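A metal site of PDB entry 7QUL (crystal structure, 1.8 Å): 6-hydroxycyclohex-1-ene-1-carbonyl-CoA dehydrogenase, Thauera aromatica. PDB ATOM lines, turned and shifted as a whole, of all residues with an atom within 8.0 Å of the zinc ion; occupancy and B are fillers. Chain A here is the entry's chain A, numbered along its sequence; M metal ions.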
ATOM      1  N   MET A  92      -0.110  28.737  19.184  1.00  0.00           N
ATOM      2  CA  MET A  92      -1.018  29.917  19.268  1.00  0.00           C
ATOM      3  C   MET A  92      -1.705  30.011  17.902  1.00  0.00           C
ATOM      4  O   MET A  92      -1.030  30.293  16.907  1.00  0.00           O
ATOM      5  CB  MET A  92      -0.198  31.178  19.576  1.00  0.00           C
ATOM      6  CG  MET A  92       0.742  31.022  20.773  1.00  0.00           C
ATOM      7  SD  MET A  92       2.406  31.704  20.521  1.00  0.00           S
ATOM      8  CE  MET A  92       3.035  31.734  22.203  1.00  0.00           C
ATOM      9  N   PRO A  93      -2.987  29.615  17.768  1.00  0.00           N
ATOM     10  CA  PRO A  93      -3.731  29.778  16.509  1.00  0.00           C
ATOM     11  C   PRO A  93      -4.061  31.256  16.219  1.00  0.00           C
ATOM     12  O   PRO A  93      -4.054  32.090  17.133  1.00  0.00           O
ATOM     13  CB  PRO A  93      -5.015  28.961  16.711  1.00  0.00           C
ATOM     14  CG  PRO A  93      -4.664  28.001  17.854  1.00  0.00           C
ATOM     15  CD  PRO A  93      -3.755  28.814  18.741  1.00  0.00           C
ATOM     16  N   CYS A  94      -4.316  31.580  14.956  1.00  0.00           N
ATOM     17  CA  CYS A  94      -4.384  33.007  14.549  1.00  0.00           C
ATOM     18  C   CYS A  94      -5.597  33.611  15.255  1.00  0.00           C
ATOM     19  O   CYS A  94      -5.519  34.789  15.609  1.00  0.00           O
ATOM     20  CB  CYS A  94      -4.365  33.175  13.028  1.00  0.00           C
ATOM     21  SG  CYS A  94      -5.977  32.947  12.243  1.00  0.00           S
ATOM     22  N   GLY A  95      -6.628  32.803  15.529  1.00  0.00           N
ATOM     23  CA  GLY A  95      -7.806  33.242  16.293  1.00  0.00           C
ATOM     24  C   GLY A  95      -8.681  34.172  15.478  1.00  0.00           C
ATOM     25  O   GLY A  95      -9.704  34.626  16.008  1.00  0.00           O
ATOM     26  N   THR A  96      -8.296  34.461  14.233  1.00  0.00           N
ATOM     27  CA  THR A  96      -8.976  35.442  13.346  1.00  0.00           C
ATOM     28  C   THR A  96      -9.420  34.748  12.049  1.00  0.00           C
ATOM     29  O   THR A  96     -10.498  35.149  11.576  1.00  0.00           O
ATOM     30  CB  THR A  96      -8.143  36.737  13.215  1.00  0.00           C
ATOM     31  OG1 THR A  96      -6.984  36.549  12.410  1.00  0.00           O
ATOM     32  CG2 THR A  96      -7.678  37.291  14.536  1.00  0.00           C
ATOM     33  N   CYS A  97      -8.712  33.700  11.570  1.00  0.00           N
ATOM     34  CA  CYS A  97      -9.074  32.901  10.343  1.00  0.00           C
ATOM     35  C   CYS A  97     -10.368  32.158  10.606  1.00  0.00           C
ATOM     36  O   CYS A  97     -10.752  32.036  11.781  1.00  0.00           O
ATOM     37  CB  CYS A  97      -8.003  31.929   9.831  1.00  0.00           C
ATOM     38  SG  CYS A  97      -7.852  30.319  10.676  1.00  0.00           S
ATOM     39  N   GLU A  98     -11.041  31.758   9.523  1.00  0.00           N
ATOM     40  CA  GLU A  98     -12.375  31.094   9.545  1.00  0.00           C
ATOM     41  C   GLU A  98     -12.250  29.752  10.262  1.00  0.00           C
ATOM     42  O   GLU A  98     -13.272  29.295  10.834  1.00  0.00           O
ATOM     43  CB  GLU A  98     -12.919  30.941   8.122  1.00  0.00           C
ATOM     44  N   LEU A  99     -11.065  29.136  10.223  1.00  0.00           N
ATOM     45  CA  LEU A  99     -10.796  27.813  10.862  1.00  0.00           C
ATOM     46  C   LEU A  99     -10.720  27.957  12.383  1.00  0.00           C
ATOM     47  O   LEU A  99     -11.190  27.043  13.083  1.00  0.00           O
ATOM     48  CB  LEU A  99      -9.499  27.199  10.311  1.00  0.00           C
ATOM     49  CG  LEU A  99      -9.618  26.429   9.009  1.00  0.00           C
ATOM     50  CD1 LEU A  99      -8.328  25.663   8.728  1.00  0.00           C
ATOM     51  CD2 LEU A  99     -10.807  25.476   9.033  1.00  0.00           C
ATOM     52  N   CYS A 100     -10.170  29.082  12.862  1.00  0.00           N
ATOM     53  CA  CYS A 100     -10.157  29.463  14.302  1.00  0.00           C
ATOM     54  C   CYS A 100     -11.534  29.979  14.747  1.00  0.00           C
ATOM     55  O   CYS A 100     -11.962  29.550  15.836  1.00  0.00           O
ATOM     56  CB  CYS A 100      -9.112  30.526  14.595  1.00  0.00           C
ATOM     57  SG  CYS A 100      -7.444  29.867  14.349  1.00  0.00           S
ATOM     58  N   THR A 101     -12.171  30.868  13.967  1.00  0.00           N
ATOM     59  CA  THR A 101     -13.568  31.360  14.196  1.00  0.00           C
ATOM     60  C   THR A 101     -14.471  30.190  14.591  1.00  0.00           C
ATOM     61  O   THR A 101     -15.204  30.321  15.590  1.00  0.00           O
ATOM     62  CB  THR A 101     -14.249  31.921  12.938  1.00  0.00           C
ATOM     63  OG1 THR A 101     -14.313  30.824  12.033  1.00  0.00           O
ATOM     64  CG2 THR A 101     -13.573  33.127  12.329  1.00  0.00           C
ATOM     65  N   GLY A 105      -8.875  25.003  15.142  1.00  0.00           N
ATOM     66  CA  GLY A 105      -7.767  25.923  15.443  1.00  0.00           C
ATOM     67  C   GLY A 105      -6.444  25.202  15.535  1.00  0.00           C
ATOM     68  O   GLY A 105      -5.381  25.850  15.281  1.00  0.00           O
ATOM     69  N   THR A 106      -6.454  23.926  15.918  1.00  0.00           N
ATOM     70  CA  THR A 106      -5.223  23.140  16.178  1.00  0.00           C
ATOM     71  C   THR A 106      -4.381  23.110  14.891  1.00  0.00           C
ATOM     72  O   THR A 106      -3.143  23.262  15.034  1.00  0.00           O
ATOM     73  CB  THR A 106      -5.541  21.754  16.751  1.00  0.00           C
ATOM     74  OG1 THR A 106      -6.699  21.245  16.078  1.00  0.00           O
ATOM     75  CG2 THR A 106      -5.813  21.832  18.243  1.00  0.00           C
ATOM     76  N   ILE A 107      -5.046  23.028  13.731  1.00  0.00           N
ATOM     77  CA  ILE A 107      -4.406  22.924  12.379  1.00  0.00           C
ATOM     78  C   ILE A 107      -4.261  24.294  11.692  1.00  0.00           C
ATOM     79  O   ILE A 107      -3.662  24.294  10.588  1.00  0.00           O
ATOM     80  CB  ILE A 107      -5.129  21.902  11.470  1.00  0.00           C
ATOM     81  CG1 ILE A 107      -6.667  21.927  11.560  1.00  0.00           C
ATOM     82  CG2 ILE A 107      -4.591  20.512  11.768  1.00  0.00           C
ATOM     83  CD1 ILE A 107      -7.330  23.227  11.159  1.00  0.00           C
ATOM     84  N   CYS A 108      -4.737  25.399  12.295  1.00  0.00           N
ATOM     85  CA  CYS A 108      -4.678  26.799  11.734  1.00  0.00           C
ATOM     86  C   CYS A 108      -3.422  26.996  10.885  1.00  0.00           C
ATOM     87  O   CYS A 108      -2.324  26.745  11.404  1.00  0.00           O
ATOM     88  CB  CYS A 108      -4.736  27.853  12.846  1.00  0.00           C
ATOM     89  SG  CYS A 108      -4.363  29.548  12.327  1.00  0.00           S
ATOM     90  N   ARG A 109      -3.574  27.473   9.648  1.00  0.00           N
ATOM     91  CA  ARG A 109      -2.481  27.544   8.646  1.00  0.00           C
ATOM     92  C   ARG A 109      -1.498  28.618   9.090  1.00  0.00           C
ATOM     93  O   ARG A 109      -0.339  28.604   8.624  1.00  0.00           O
ATOM     94  CB  ARG A 109      -3.044  27.816   7.235  1.00  0.00           C
ATOM     95  N   ASP A 110      -1.952  29.514   9.969  1.00  0.00           N
ATOM     96  CA  ASP A 110      -1.208  30.713  10.419  1.00  0.00           C
ATOM     97  C   ASP A 110      -0.844  30.538  11.903  1.00  0.00           C
ATOM     98  O   ASP A 110      -0.453  31.522  12.491  1.00  0.00           O
ATOM     99  CB  ASP A 110      -1.994  31.986  10.098  1.00  0.00           C
ATOM    100  CG  ASP A 110      -2.149  32.226   8.602  1.00  0.00           C
ATOM    101  OD1 ASP A 110      -1.277  31.742   7.837  1.00  0.00           O
ATOM    102  OD2 ASP A 110      -3.156  32.868   8.203  1.00  0.00           O
ATOM    103  N   GLN A 111      -0.901  29.323  12.451  1.00  0.00           N
ATOM    104  CA  GLN A 111      -0.535  29.042  13.875  1.00  0.00           C
ATOM    105  C   GLN A 111       0.977  29.210  14.099  1.00  0.00           C
ATOM    106  O   GLN A 111       1.782  28.854  13.184  1.00  0.00           O
ATOM    107  CB  GLN A 111      -0.935  27.639  14.310  1.00  0.00           C
ATOM    108  CG  GLN A 111      -0.083  26.534  13.698  1.00  0.00           C
ATOM    109  CD  GLN A 111      -0.616  25.164  14.005  1.00  0.00           C
ATOM    110  OE1 GLN A 111      -0.005  24.391  14.734  1.00  0.00           O
ATOM    111  NE2 GLN A 111      -1.767  24.848  13.449  1.00  0.00           N
ATOM    112  N   ARG A 131      -2.022  36.673  22.800  1.00  0.00           N
ATOM    113  CA  ARG A 131      -3.215  35.830  22.512  1.00  0.00           C
ATOM    114  C   ARG A 131      -3.092  34.432  23.171  1.00  0.00           C
ATOM    115  O   ARG A 131      -2.028  33.776  23.076  1.00  0.00           O
ATOM    116  CB  ARG A 131      -3.548  35.791  21.014  1.00  0.00           C
ATOM    117  CG  ARG A 131      -2.510  35.137  20.106  1.00  0.00           C
ATOM    118  CD  ARG A 131      -3.076  35.051  18.680  1.00  0.00           C
ATOM    119  NE  ARG A 131      -2.133  34.578  17.677  1.00  0.00           N
ATOM    120  CZ  ARG A 131      -1.142  35.308  17.141  1.00  0.00           C
ATOM    121  NH1 ARG A 131      -0.928  36.554  17.544  1.00  0.00           N
ATOM    122  NH2 ARG A 131      -0.355  34.776  16.223  1.00  0.00           N
HETATM  123 ZN    ZN M   1      -6.434  30.673  12.391  1.00  0.00          ZN
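The side-chain sulfur of Cys 97 sits close to the backbone NH of Leu 99, 3.5 Å away. SG of Cys 94 lies close to N of Thr 96, at 3.4 Å. N of Gly 95 sits close to SG of Cys 100, at 3.3 Å. The backbone NH (N) of Asp 110 sits close to the side-chain sulfur (SG) of Cys 108 (3.4 Å). O of Cys 108 is in hydrogen-bond range of NE2 of Gln 111, at 2.8 Å.
N of Gly 95 touches the zinc ion, 3.8 Å away. Five residues have an atom within 4 Å of the zinc ion: Cys 94, Gly 95, Cys 97, Cys 100 and Cys 108. The nearest printed residue that does not touch the zinc ion is Pro 93 (4.5 Å).
The zinc ion is bound by the side-chain sulfur (SG) of Cys 97 (2.3 Å), the side-chain sulfur (SG) of Cys 94 (2.3 Å), the side-chain sulfur (SG) of Cys 100 (2.3 Å) and the side-chain sulfur (SG) of Cys 108 (2.4 Å).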
